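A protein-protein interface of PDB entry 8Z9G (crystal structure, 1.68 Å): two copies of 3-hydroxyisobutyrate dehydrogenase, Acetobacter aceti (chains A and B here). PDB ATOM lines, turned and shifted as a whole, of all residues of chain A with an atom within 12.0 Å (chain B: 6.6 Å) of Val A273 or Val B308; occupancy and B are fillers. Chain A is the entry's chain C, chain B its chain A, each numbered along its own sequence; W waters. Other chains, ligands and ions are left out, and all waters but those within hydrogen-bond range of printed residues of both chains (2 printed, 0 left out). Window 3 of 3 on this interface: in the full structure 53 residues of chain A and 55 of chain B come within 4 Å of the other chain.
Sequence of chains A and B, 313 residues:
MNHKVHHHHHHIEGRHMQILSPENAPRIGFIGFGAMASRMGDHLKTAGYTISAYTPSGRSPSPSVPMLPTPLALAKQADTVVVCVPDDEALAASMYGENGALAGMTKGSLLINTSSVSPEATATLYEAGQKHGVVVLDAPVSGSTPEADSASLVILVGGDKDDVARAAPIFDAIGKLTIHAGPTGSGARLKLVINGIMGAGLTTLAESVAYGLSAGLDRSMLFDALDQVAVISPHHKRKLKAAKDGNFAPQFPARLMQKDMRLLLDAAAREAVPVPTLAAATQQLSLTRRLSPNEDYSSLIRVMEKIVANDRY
The side-chain hydroxyl (OG1) of Thr A277 lies within hydrogen-bond range of the side-chain carboxylate (OE2) of Glu B207. The backbone NH (N) of Leu A278 is in hydrogen-bond range of the side-chain carboxylate (OE1) of Glu B207, 3.1 Å away. The guanidinium group of Arg A189 lies within hydrogen-bond range of the backbone carbonyl oxygen of Ala B215. The side-chain carboxylate of Glu A271 sits close to the backbone carbonyl oxygen of Ser B214 (3.4 Å). O of Val A275 lies close to OE1 of Glu B207. N of Pro A276 lies close to OE1 of Glu B207, 3.5 Å away.
The backbone carbonyl oxygen (O) of Ala B210 lies close to the side-chain hydroxyl (OG) of Ser B214 (3.5 Å). OG of Ser B214 lies within hydrogen-bond range of O of Tyr B211, 2.6 Å away. The backbone NH of Val A273 lies within hydrogen-bond range of the backbone carbonyl oxygen of Ala A268 (3.0 Å). The backbone carbonyl oxygen (O) of Leu A278 lies within hydrogen-bond range of the side-chain hydroxyl (OG1) of Thr A282, at 2.9 Å.
Tyr B211 touches Arg A189 (OH to CG, 3.7 Å). Leu A192 touches Tyr B211 (CD1 to OH, 3.5 Å). CD2 of Tyr B211 touches CG2 of Val A193, 3.8 Å away. CB of Ala A267 touches OH of Tyr B211, at 3.5 Å. Tyr B211 touches Ala A268. Tyr B211 touches Glu A271. OE2 of Glu A271 touches CA of Ala B215, at 3.8 Å. CB of Ala B210 touches CG1 of Val A273, 3.9 Å away. Val B308 touches Val A273 (CG1 to CG1, 3.8 Å). Pro A274 touches Met B304.
Of the printed residues of chain B, Pro A119 touches Tyr B211 (3.9 Å). Arg A270 touches none of the printed residues of chain B. Of the printed residues of chain B, Glu A271 touches Tyr B211, Ser B214 and Ala B215. Of chain B, only Ala B210 (3.9 Å), Ser B214 (3.1 Å) and Val B308 (3.8 Å) come within 4 Å of Val A273. Of the printed residues of chain B, Val A275 touches Glu B207 (3.1 Å). No residue of chain A comes within 4 Å of Leu B213. Ser B214 touches two residues of chain A. Met B304 touches one residue of chain A. Glu B305 touches none of the printed residues of chain A. Of chain A, only Val A273 (3.8 Å) comes within 4 Å of Val B308. No residue of chain A comes within 4 Å of Ala B309. The nearest residue of chain A that does not touch Val B308 is Pro A274 (5.9 Å).
Among the printed residues, no Asp or Glu carboxylate lies within 4 Å of a Lys or Arg side-chain nitrogen of the other chain.
No position is printed for both chains.
Water W1 lies within hydrogen-bond range of OE2 of Glu A271 (2.6 Å), NH2 of Arg A189 (3.0 Å) and O of Ala B215 (3.2 Å). Water W2 bridges the side-chain hydroxyl of Tyr B211 and the side-chain carboxylate of Glu A271.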
ATOM      1  N   PRO A 119      -2.334   1.204  -4.878  1.00  0.00           N
ATOM      2  CA  PRO A 119      -2.372   0.459  -6.156  1.00  0.00           C
ATOM      3  C   PRO A 119      -3.782   0.188  -6.666  1.00  0.00           C
ATOM      4  O   PRO A 119      -3.995   0.127  -7.891  1.00  0.00           O
ATOM      5  CB  PRO A 119      -1.643  -0.849  -5.809  1.00  0.00           C
ATOM      6  CG  PRO A 119      -0.681  -0.436  -4.710  1.00  0.00           C
ATOM      7  CD  PRO A 119      -1.500   0.527  -3.867  1.00  0.00           C
ATOM      8  N   ARG A 189       3.658   1.839  -7.061  1.00  0.00           N
ATOM      9  CA  ARG A 189       4.341   0.855  -6.221  1.00  0.00           C
ATOM     10  C   ARG A 189       5.725   1.335  -5.797  1.00  0.00           C
ATOM     11  O   ARG A 189       6.105   1.182  -4.634  1.00  0.00           O
ATOM     12  CB  ARG A 189       4.440  -0.477  -6.957  1.00  0.00           C
ATOM     13  CG  ARG A 189       3.120  -1.224  -7.044  1.00  0.00           C
ATOM     14  CD  ARG A 189       3.096  -2.148  -8.261  1.00  0.00           C
ATOM     15  NE  ARG A 189       1.949  -3.046  -8.231  1.00  0.00           N
ATOM     16  CZ  ARG A 189       0.709  -2.689  -8.530  1.00  0.00           C
ATOM     17  NH1 ARG A 189       0.415  -1.451  -8.897  1.00  0.00           N
ATOM     18  NH2 ARG A 189      -0.261  -3.595  -8.461  1.00  0.00           N
ATOM     19  N   LEU A 192       5.446   3.729  -2.960  1.00  0.00           N
ATOM     20  CA  LEU A 192       5.222   3.062  -1.675  1.00  0.00           C
ATOM     21  C   LEU A 192       6.529   2.532  -1.081  1.00  0.00           C
ATOM     22  O   LEU A 192       6.757   2.638   0.129  1.00  0.00           O
ATOM     23  CB  LEU A 192       4.214   1.924  -1.838  1.00  0.00           C
ATOM     24  CG  LEU A 192       2.768   2.281  -2.196  1.00  0.00           C
ATOM     25  CD1 LEU A 192       1.887   1.029  -2.169  1.00  0.00           C
ATOM     26  CD2 LEU A 192       2.236   3.349  -1.288  1.00  0.00           C
ATOM     27  N   VAL A 193       7.382   1.925  -1.911  1.00  0.00           N
ATOM     28  CA  VAL A 193       8.685   1.448  -1.446  1.00  0.00           C
ATOM     29  C   VAL A 193       9.480   2.581  -0.813  1.00  0.00           C
ATOM     30  O   VAL A 193      10.052   2.440   0.276  1.00  0.00           O
ATOM     31  CB  VAL A 193       9.460   0.815  -2.615  1.00  0.00           C
ATOM     32  CG1 VAL A 193      10.887   0.470  -2.170  1.00  0.00           C
ATOM     33  CG2 VAL A 193       8.723  -0.409  -3.144  1.00  0.00           C
ATOM     34  N   MET A 261       2.137   5.584   5.047  1.00  0.00           N
ATOM     35  CA  MET A 261       2.483   4.351   5.747  1.00  0.00           C
ATOM     36  C   MET A 261       1.282   3.405   5.783  1.00  0.00           C
ATOM     37  O   MET A 261       1.423   2.199   5.556  1.00  0.00           O
ATOM     38  CB  MET A 261       2.934   4.704   7.165  1.00  0.00           C
ATOM     39  CG  MET A 261       4.370   5.205   7.372  1.00  0.00           C
ATOM     40  SD  MET A 261       5.719   4.635   6.312  1.00  0.00           S
ATOM     41  CE  MET A 261       6.217   3.216   7.289  1.00  0.00           C
ATOM     42  N   ARG A 262       0.086   3.937   6.069  1.00  0.00           N
ATOM     43  CA  ARG A 262      -1.133   3.122   6.024  1.00  0.00           C
ATOM     44  C   ARG A 262      -1.296   2.449   4.666  1.00  0.00           C
ATOM     45  O   ARG A 262      -1.586   1.248   4.585  1.00  0.00           O
ATOM     46  CB  ARG A 262      -2.377   3.973   6.341  1.00  0.00           C
ATOM     47  CG  ARG A 262      -3.675   3.170   6.179  1.00  0.00           C
ATOM     48  CD  ARG A 262      -4.936   3.925   6.628  1.00  0.00           C
ATOM     49  NE  ARG A 262      -5.126   5.157   5.875  1.00  0.00           N
ATOM     50  CZ  ARG A 262      -5.596   5.221   4.638  1.00  0.00           C
ATOM     51  NH1 ARG A 262      -5.952   4.134   3.974  1.00  0.00           N
ATOM     52  NH2 ARG A 262      -5.709   6.411   4.052  1.00  0.00           N
ATOM     53  N   LEU A 263      -1.108   3.213   3.585  1.00  0.00           N
ATOM     54  CA  LEU A 263      -1.236   2.650   2.246  1.00  0.00           C
ATOM     55  C   LEU A 263      -0.212   1.547   2.018  1.00  0.00           C
ATOM     56  O   LEU A 263      -0.520   0.515   1.416  1.00  0.00           O
ATOM     57  CB  LEU A 263      -1.063   3.748   1.192  1.00  0.00           C
ATOM     58  CG  LEU A 263      -2.148   4.828   1.077  1.00  0.00           C
ATOM     59  CD1 LEU A 263      -1.824   5.727  -0.112  1.00  0.00           C
ATOM     60  CD2 LEU A 263      -3.523   4.219   0.937  1.00  0.00           C
ATOM     61  N   LEU A 264       1.020   1.754   2.477  1.00  0.00           N
ATOM     62  CA  LEU A 264       2.053   0.756   2.236  1.00  0.00           C
ATOM     63  C   LEU A 264       1.763  -0.525   3.011  1.00  0.00           C
ATOM     64  O   LEU A 264       1.886  -1.629   2.463  1.00  0.00           O
ATOM     65  CB  LEU A 264       3.420   1.337   2.592  1.00  0.00           C
ATOM     66  CG  LEU A 264       4.542   0.317   2.736  1.00  0.00           C
ATOM     67  CD1 LEU A 264       4.873  -0.336   1.376  1.00  0.00           C
ATOM     68  CD2 LEU A 264       5.741   0.982   3.339  1.00  0.00           C
ATOM     69  N   LEU A 265       1.357  -0.402   4.278  1.00  0.00           N
ATOM     70  CA  LEU A 265       1.028  -1.601   5.048  1.00  0.00           C
ATOM     71  C   LEU A 265      -0.159  -2.347   4.455  1.00  0.00           C
ATOM     72  O   LEU A 265      -0.182  -3.587   4.452  1.00  0.00           O
ATOM     73  CB  LEU A 265       0.758  -1.234   6.502  1.00  0.00           C
ATOM     74  CG  LEU A 265       1.973  -1.090   7.395  1.00  0.00           C
ATOM     75  CD1 LEU A 265       1.455  -1.063   8.823  1.00  0.00           C
ATOM     76  CD2 LEU A 265       2.888  -2.283   7.268  1.00  0.00           C
ATOM     77  N   ASP A 266      -1.173  -1.623   3.965  1.00  0.00           N
ATOM     78  CA  ASP A 266      -2.271  -2.322   3.309  1.00  0.00           C
ATOM     79  C   ASP A 266      -1.778  -3.086   2.091  1.00  0.00           C
ATOM     80  O   ASP A 266      -2.143  -4.248   1.886  1.00  0.00           O
ATOM     81  CB  ASP A 266      -3.378  -1.346   2.918  1.00  0.00           C
ATOM     82  CG  ASP A 266      -4.570  -2.056   2.281  1.00  0.00           C
ATOM     83  OD1 ASP A 266      -4.524  -2.372   1.072  1.00  0.00           O
ATOM     84  OD2 ASP A 266      -5.508  -2.394   3.017  1.00  0.00           O
ATOM     85  N   ALA A 267      -0.935  -2.449   1.282  1.00  0.00           N
ATOM     86  CA  ALA A 267      -0.440  -3.102   0.076  1.00  0.00           C
ATOM     87  C   ALA A 267       0.440  -4.297   0.418  1.00  0.00           C
ATOM     88  O   ALA A 267       0.342  -5.345  -0.230  1.00  0.00           O
ATOM     89  CB  ALA A 267       0.323  -2.095  -0.783  1.00  0.00           C
ATOM     90  N   ALA A 268       1.271  -4.168   1.452  1.00  0.00           N
ATOM     91  CA  ALA A 268       2.119  -5.288   1.870  1.00  0.00           C
ATOM     92  C   ALA A 268       1.280  -6.447   2.395  1.00  0.00           C
ATOM     93  O   ALA A 268       1.605  -7.621   2.155  1.00  0.00           O
ATOM     94  CB  ALA A 268       3.112  -4.813   2.933  1.00  0.00           C
ATOM     95  N   ALA A 269       0.168  -6.139   3.077  1.00  0.00           N
ATOM     96  CA  ALA A 269      -0.723  -7.204   3.530  1.00  0.00           C
ATOM     97  C   ALA A 269      -1.423  -7.872   2.352  1.00  0.00           C
ATOM     98  O   ALA A 269      -1.589  -9.101   2.328  1.00  0.00           O
ATOM     99  CB  ALA A 269      -1.744  -6.648   4.535  1.00  0.00           C
ATOM    100  N   ARG A 270      -1.818  -7.087   1.351  1.00  0.00           N
ATOM    101  CA  ARG A 270      -2.491  -7.682   0.203  1.00  0.00           C
ATOM    102  C   ARG A 270      -1.562  -8.613  -0.551  1.00  0.00           C
ATOM    103  O   ARG A 270      -2.013  -9.615  -1.124  1.00  0.00           O
ATOM    104  CB  ARG A 270      -3.007  -6.592  -0.737  1.00  0.00           C
ATOM    105  CG  ARG A 270      -4.235  -5.857  -0.185  1.00  0.00           C
ATOM    106  CD  ARG A 270      -4.831  -4.945  -1.232  1.00  0.00           C
ATOM    107  NE  ARG A 270      -5.955  -4.174  -0.708  1.00  0.00           N
ATOM    108  CZ  ARG A 270      -7.234  -4.507  -0.826  1.00  0.00           C
ATOM    109  NH1 ARG A 270      -7.609  -5.630  -1.421  1.00  0.00           N
ATOM    110  NH2 ARG A 270      -8.163  -3.684  -0.345  1.00  0.00           N
ATOM    111  N   GLU A 271      -0.270  -8.287  -0.589  1.00  0.00           N
ATOM    112  CA  GLU A 271       0.723  -9.160  -1.215  1.00  0.00           C
ATOM    113  C   GLU A 271       1.222 -10.259  -0.289  1.00  0.00           C
ATOM    114  O   GLU A 271       2.005 -11.109  -0.743  1.00  0.00           O
ATOM    115  CB  GLU A 271       1.943  -8.363  -1.711  1.00  0.00           C
ATOM    116  CG  GLU A 271       1.626  -7.168  -2.620  1.00  0.00           C
ATOM    117  CD  GLU A 271       1.115  -7.571  -3.992  1.00  0.00           C
ATOM    118  OE1 GLU A 271       1.099  -8.781  -4.300  1.00  0.00           O
ATOM    119  OE2 GLU A 271       0.717  -6.670  -4.765  1.00  0.00           O
ATOM    120  N   ALA A 272       0.803 -10.257   0.984  1.00  0.00           N
ATOM    121  CA  ALA A 272       1.264 -11.211   1.997  1.00  0.00           C
ATOM    122  C   ALA A 272       2.782 -11.214   2.138  1.00  0.00           C
ATOM    123  O   ALA A 272       3.420 -12.268   2.112  1.00  0.00           O
ATOM    124  CB  ALA A 272       0.755 -12.627   1.709  1.00  0.00           C
ATOM    125  N   VAL A 273       3.363 -10.033   2.313  1.00  0.00           N
ATOM    126  CA  VAL A 273       4.794  -9.876   2.533  1.00  0.00           C
ATOM    127  C   VAL A 273       4.988  -9.431   3.975  1.00  0.00           C
ATOM    128  O   VAL A 273       4.475  -8.367   4.345  1.00  0.00           O
ATOM    129  CB  VAL A 273       5.406  -8.847   1.576  1.00  0.00           C
ATOM    130  CG1 VAL A 273       6.945  -8.842   1.722  1.00  0.00           C
ATOM    131  CG2 VAL A 273       4.993  -9.181   0.196  1.00  0.00           C
ATOM    132  N   PRO A 274       5.717 -10.180   4.807  1.00  0.00           N
ATOM    133  CA  PRO A 274       5.885  -9.778   6.216  1.00  0.00           C
ATOM    134  C   PRO A 274       6.883  -8.633   6.345  1.00  0.00           C
ATOM    135  O   PRO A 274       8.044  -8.759   5.955  1.00  0.00           O
ATOM    136  CB  PRO A 274       6.389 -11.055   6.896  1.00  0.00           C
ATOM    137  CG  PRO A 274       6.999 -11.895   5.794  1.00  0.00           C
ATOM    138  CD  PRO A 274       6.365 -11.475   4.492  1.00  0.00           C
ATOM    139  N   VAL A 275       6.423  -7.499   6.877  1.00  0.00           N
ATOM    140  CA  VAL A 275       7.306  -6.339   6.983  1.00  0.00           C
ATOM    141  C   VAL A 275       7.281  -5.771   8.407  1.00  0.00           C
ATOM    142  O   VAL A 275       6.770  -4.661   8.625  1.00  0.00           O
ATOM    143  CB  VAL A 275       6.944  -5.276   5.929  1.00  0.00           C
ATOM    144  CG1 VAL A 275       7.278  -5.801   4.518  1.00  0.00           C
ATOM    145  CG2 VAL A 275       5.443  -4.848   5.964  1.00  0.00           C
ATOM    146  N   PRO A 276       7.859  -6.474   9.396  1.00  0.00           N
ATOM    147  CA  PRO A 276       7.712  -6.026  10.798  1.00  0.00           C
ATOM    148  C   PRO A 276       8.336  -4.673  11.097  1.00  0.00           C
ATOM    149  O   PRO A 276       7.786  -3.936  11.933  1.00  0.00           O
ATOM    150  CB  PRO A 276       8.392  -7.149  11.606  1.00  0.00           C
ATOM    151  CG  PRO A 276       9.228  -7.913  10.598  1.00  0.00           C
ATOM    152  CD  PRO A 276       8.521  -7.787   9.295  1.00  0.00           C
ATOM    153  N   THR A 277       9.471  -4.326  10.475  1.00  0.00           N
ATOM    154  CA  THR A 277      10.075  -3.016  10.753  1.00  0.00           C
ATOM    155  C   THR A 277       9.179  -1.892  10.240  1.00  0.00           C
ATOM    156  O   THR A 277       8.965  -0.890  10.933  1.00  0.00           O
ATOM    157  CB  THR A 277      11.480  -2.919  10.139  1.00  0.00           C
ATOM    158  OG1 THR A 277      12.208  -4.125  10.423  1.00  0.00           O
ATOM    159  CG2 THR A 277      12.235  -1.735  10.748  1.00  0.00           C
ATOM    160  N   LEU A 278       8.626  -2.054   9.034  1.00  0.00           N
ATOM    161  CA  LEU A 278       7.715  -1.058   8.484  1.00  0.00           C
ATOM    162  C   LEU A 278       6.435  -0.974   9.302  1.00  0.00           C
ATOM    163  O   LEU A 278       5.870   0.113   9.469  1.00  0.00           O
ATOM    164  CB  LEU A 278       7.377  -1.402   7.023  1.00  0.00           C
ATOM    165  CG  LEU A 278       8.589  -1.489   6.093  1.00  0.00           C
ATOM    166  CD1 LEU A 278       8.154  -1.822   4.694  1.00  0.00           C
ATOM    167  CD2 LEU A 278       9.330  -0.167   6.073  1.00  0.00           C
ATOM    168  N   ALA A 279       5.955  -2.119   9.802  1.00  0.00           N
ATOM    169  CA  ALA A 279       4.731  -2.140  10.604  1.00  0.00           C
ATOM    170  C   ALA A 279       4.911  -1.391  11.914  1.00  0.00           C
ATOM    171  O   ALA A 279       4.020  -0.626  12.323  1.00  0.00           O
ATOM    172  CB  ALA A 279       4.326  -3.582  10.902  1.00  0.00           C
ATOM    173  N   ALA A 280       6.036  -1.629  12.598  1.00  0.00           N
ATOM    174  CA  ALA A 280       6.336  -0.890  13.823  1.00  0.00           C
ATOM    175  C   ALA A 280       6.430   0.605  13.553  1.00  0.00           C
ATOM    176  O   ALA A 280       5.935   1.427  14.343  1.00  0.00           O
ATOM    177  CB  ALA A 280       7.653  -1.384  14.428  1.00  0.00           C
ATOM    178  N   THR A 282       5.016   2.370  11.255  1.00  0.00           N
ATOM    179  CA  THR A 282       3.678   2.906  11.038  1.00  0.00           C
ATOM    180  C   THR A 282       2.996   3.223  12.360  1.00  0.00           C
ATOM    181  O   THR A 282       2.342   4.262  12.488  1.00  0.00           O
ATOM    182  CB  THR A 282       2.852   1.903  10.226  1.00  0.00           C
ATOM    183  OG1 THR A 282       3.509   1.639   8.978  1.00  0.00           O
ATOM    184  CG2 THR A 282       1.456   2.451   9.941  1.00  0.00           C
ATOM    185  N   GLU B 207      12.847  -4.938   3.749  1.00  0.00           N
ATOM    186  CA  GLU B 207      11.402  -5.127   3.698  1.00  0.00           C
ATOM    187  C   GLU B 207      10.773  -4.280   2.606  1.00  0.00           C
ATOM    188  O   GLU B 207       9.839  -4.721   1.936  1.00  0.00           O
ATOM    189  CB  GLU B 207      10.769  -4.808   5.061  1.00  0.00           C
ATOM    190  CG  GLU B 207      11.315  -5.686   6.143  1.00  0.00           C
ATOM    191  CD  GLU B 207      10.853  -5.296   7.523  1.00  0.00           C
ATOM    192  OE1 GLU B 207      10.001  -4.398   7.621  1.00  0.00           O
ATOM    193  OE2 GLU B 207      11.417  -5.829   8.503  1.00  0.00           O
ATOM    194  N   VAL B 209      12.195  -3.232  -0.216  1.00  0.00           N
ATOM    195  CA  VAL B 209      12.518  -3.908  -1.470  1.00  0.00           C
ATOM    196  C   VAL B 209      11.624  -5.119  -1.659  1.00  0.00           C
ATOM    197  O   VAL B 209      11.133  -5.381  -2.764  1.00  0.00           O
ATOM    198  CB  VAL B 209      14.009  -4.294  -1.486  1.00  0.00           C
ATOM    199  CG1 VAL B 209      14.309  -5.261  -2.622  1.00  0.00           C
ATOM    200  CG2 VAL B 209      14.867  -3.048  -1.615  1.00  0.00           C
ATOM    201  N   ALA B 210      11.399  -5.884  -0.583  1.00  0.00           N
ATOM    202  CA  ALA B 210      10.567  -7.073  -0.690  1.00  0.00           C
ATOM    203  C   ALA B 210       9.151  -6.722  -1.108  1.00  0.00           C
ATOM    204  O   ALA B 210       8.571  -7.400  -1.962  1.00  0.00           O
ATOM    205  CB  ALA B 210      10.550  -7.853   0.625  1.00  0.00           C
ATOM    206  N   TYR B 211       8.559  -5.679  -0.506  1.00  0.00           N
ATOM    207  CA  TYR B 211       7.251  -5.256  -0.984  1.00  0.00           C
ATOM    208  C   TYR B 211       7.304  -4.968  -2.484  1.00  0.00           C
ATOM    209  O   TYR B 211       6.477  -5.468  -3.260  1.00  0.00           O
ATOM    210  CB  TYR B 211       6.734  -4.013  -0.224  1.00  0.00           C
ATOM    211  CG  TYR B 211       5.588  -3.459  -1.022  1.00  0.00           C
ATOM    212  CD1 TYR B 211       4.415  -4.182  -1.158  1.00  0.00           C
ATOM    213  CD2 TYR B 211       5.728  -2.294  -1.765  1.00  0.00           C
ATOM    214  CE1 TYR B 211       3.389  -3.746  -1.974  1.00  0.00           C
ATOM    215  CE2 TYR B 211       4.737  -1.863  -2.579  1.00  0.00           C
ATOM    216  CZ  TYR B 211       3.559  -2.581  -2.685  1.00  0.00           C
ATOM    217  OH  TYR B 211       2.555  -2.152  -3.518  1.00  0.00           O
ATOM    218  N   LEU B 213       9.224  -5.972  -4.889  1.00  0.00           N
ATOM    219  CA  LEU B 213       9.320  -7.175  -5.719  1.00  0.00           C
ATOM    220  C   LEU B 213       8.018  -7.957  -5.707  1.00  0.00           C
ATOM    221  O   LEU B 213       7.595  -8.488  -6.747  1.00  0.00           O
ATOM    222  CB  LEU B 213      10.472  -8.053  -5.226  1.00  0.00           C
ATOM    223  CG  LEU B 213      11.845  -7.394  -5.278  1.00  0.00           C
ATOM    224  CD1 LEU B 213      12.880  -8.235  -4.527  1.00  0.00           C
ATOM    225  CD2 LEU B 213      12.238  -7.175  -6.744  1.00  0.00           C
ATOM    226  N   SER B 214       7.357  -8.034  -4.545  1.00  0.00           N
ATOM    227  CA  SER B 214       6.114  -8.792  -4.448  1.00  0.00           C
ATOM    228  C   SER B 214       5.021  -8.148  -5.272  1.00  0.00           C
ATOM    229  O   SER B 214       4.132  -8.837  -5.786  1.00  0.00           O
ATOM    230  CB  SER B 214       5.634  -8.890  -3.009  1.00  0.00           C
ATOM    231  OG  SER B 214       5.126  -7.628  -2.531  1.00  0.00           O
ATOM    232  N   ALA B 215       5.102  -6.838  -5.440  1.00  0.00           N
ATOM    233  CA  ALA B 215       4.136  -6.079  -6.211  1.00  0.00           C
ATOM    234  C   ALA B 215       4.467  -6.056  -7.698  1.00  0.00           C
ATOM    235  O   ALA B 215       3.778  -5.378  -8.458  1.00  0.00           O
ATOM    236  CB  ALA B 215       4.046  -4.654  -5.654  1.00  0.00           C
ATOM    237  N   VAL B 303      17.363 -12.940   2.008  1.00  0.00           N
ATOM    238  CA  VAL B 303      16.344 -13.692   2.742  1.00  0.00           C
ATOM    239  C   VAL B 303      14.946 -13.233   2.344  1.00  0.00           C
ATOM    240  O   VAL B 303      14.068 -14.050   2.031  1.00  0.00           O
ATOM    241  CB  VAL B 303      16.557 -13.537   4.260  1.00  0.00           C
ATOM    242  CG1 VAL B 303      15.379 -14.136   5.034  1.00  0.00           C
ATOM    243  CG2 VAL B 303      17.863 -14.188   4.692  1.00  0.00           C
ATOM    244  N   MET B 304      14.712 -11.918   2.391  1.00  0.00           N
ATOM    245  CA  MET B 304      13.414 -11.365   2.008  1.00  0.00           C
ATOM    246  C   MET B 304      13.080 -11.637   0.549  1.00  0.00           C
ATOM    247  O   MET B 304      11.923 -11.897   0.221  1.00  0.00           O
ATOM    248  CB  MET B 304      13.379  -9.861   2.300  1.00  0.00           C
ATOM    249  CG  MET B 304      13.417  -9.449   3.780  1.00  0.00           C
ATOM    250  SD  MET B 304      12.166 -10.257   4.806  1.00  0.00           S
ATOM    251  CE  MET B 304      10.647  -9.773   3.990  1.00  0.00           C
ATOM    252  N   GLU B 305      14.069 -11.564  -0.342  1.00  0.00           N
ATOM    253  CA  GLU B 305      13.808 -11.901  -1.742  1.00  0.00           C
ATOM    254  C   GLU B 305      13.322 -13.339  -1.879  1.00  0.00           C
ATOM    255  O   GLU B 305      12.426 -13.631  -2.685  1.00  0.00           O
ATOM    256  CB  GLU B 305      15.071 -11.693  -2.581  1.00  0.00           C
ATOM    257  CG  GLU B 305      15.451 -10.237  -2.811  1.00  0.00           C
ATOM    258  CD  GLU B 305      16.511 -10.101  -3.904  1.00  0.00           C
ATOM    259  OE1 GLU B 305      16.152 -10.243  -5.088  1.00  0.00           O
ATOM    260  OE2 GLU B 305      17.693  -9.861  -3.586  1.00  0.00           O
ATOM    261  N   LYS B 306      13.932 -14.262  -1.125  1.00  0.00           N
ATOM    262  CA  LYS B 306      13.514 -15.656  -1.184  1.00  0.00           C
ATOM    263  C   LYS B 306      12.125 -15.857  -0.585  1.00  0.00           C
ATOM    264  O   LYS B 306      11.354 -16.679  -1.086  1.00  0.00           O
ATOM    265  CB  LYS B 306      14.558 -16.537  -0.490  1.00  0.00           C
ATOM    266  CG  LYS B 306      15.944 -16.406  -1.100  1.00  0.00           C
ATOM    267  CD  LYS B 306      16.718 -17.724  -1.062  1.00  0.00           C
ATOM    268  CE  LYS B 306      18.216 -17.484  -1.234  1.00  0.00           C
ATOM    269  NZ  LYS B 306      18.552 -17.212  -2.653  1.00  0.00           N
ATOM    270  N   ILE B 307      11.760 -15.098   0.456  1.00  0.00           N
ATOM    271  CA  ILE B 307      10.393 -15.205   0.960  1.00  0.00           C
ATOM    272  C   ILE B 307       9.392 -14.825  -0.125  1.00  0.00           C
ATOM    273  O   ILE B 307       8.370 -15.497  -0.318  1.00  0.00           O
ATOM    274  CB  ILE B 307      10.216 -14.339   2.221  1.00  0.00           C
ATOM    275  CG1 ILE B 307      11.015 -14.932   3.378  1.00  0.00           C
ATOM    276  CG2 ILE B 307       8.729 -14.214   2.561  1.00  0.00           C
ATOM    277  CD1 ILE B 307      11.153 -13.998   4.597  1.00  0.00           C
ATOM    278  N   VAL B 308       9.666 -13.747  -0.859  1.00  0.00           N
ATOM    279  CA  VAL B 308       8.675 -13.296  -1.825  1.00  0.00           C
ATOM    280  C   VAL B 308       8.683 -14.161  -3.079  1.00  0.00           C
ATOM    281  O   VAL B 308       7.658 -14.247  -3.752  1.00  0.00           O
ATOM    282  CB  VAL B 308       8.847 -11.801  -2.154  1.00  0.00           C
ATOM    283  CG1 VAL B 308       8.679 -10.974  -0.883  1.00  0.00           C
ATOM    284  CG2 VAL B 308      10.179 -11.528  -2.741  1.00  0.00           C
ATOM    285  N   ALA B 309       9.783 -14.846  -3.367  1.00  0.00           N
ATOM    286  CA  ALA B 309       9.818 -15.814  -4.456  1.00  0.00           C
ATOM    287  C   ALA B 309       8.957 -17.034  -4.114  1.00  0.00           C
ATOM    288  O   ALA B 309       8.872 -17.447  -2.945  1.00  0.00           O
ATOM    289  CB  ALA B 309      11.248 -16.231  -4.752  1.00  0.00           C
HETATM  290  O   HOH W   1       0.830  -6.096  -7.329  1.00  0.00           O
HETATM  291  O   HOH W   2       0.607  -3.940  -4.166  1.00  0.00           O
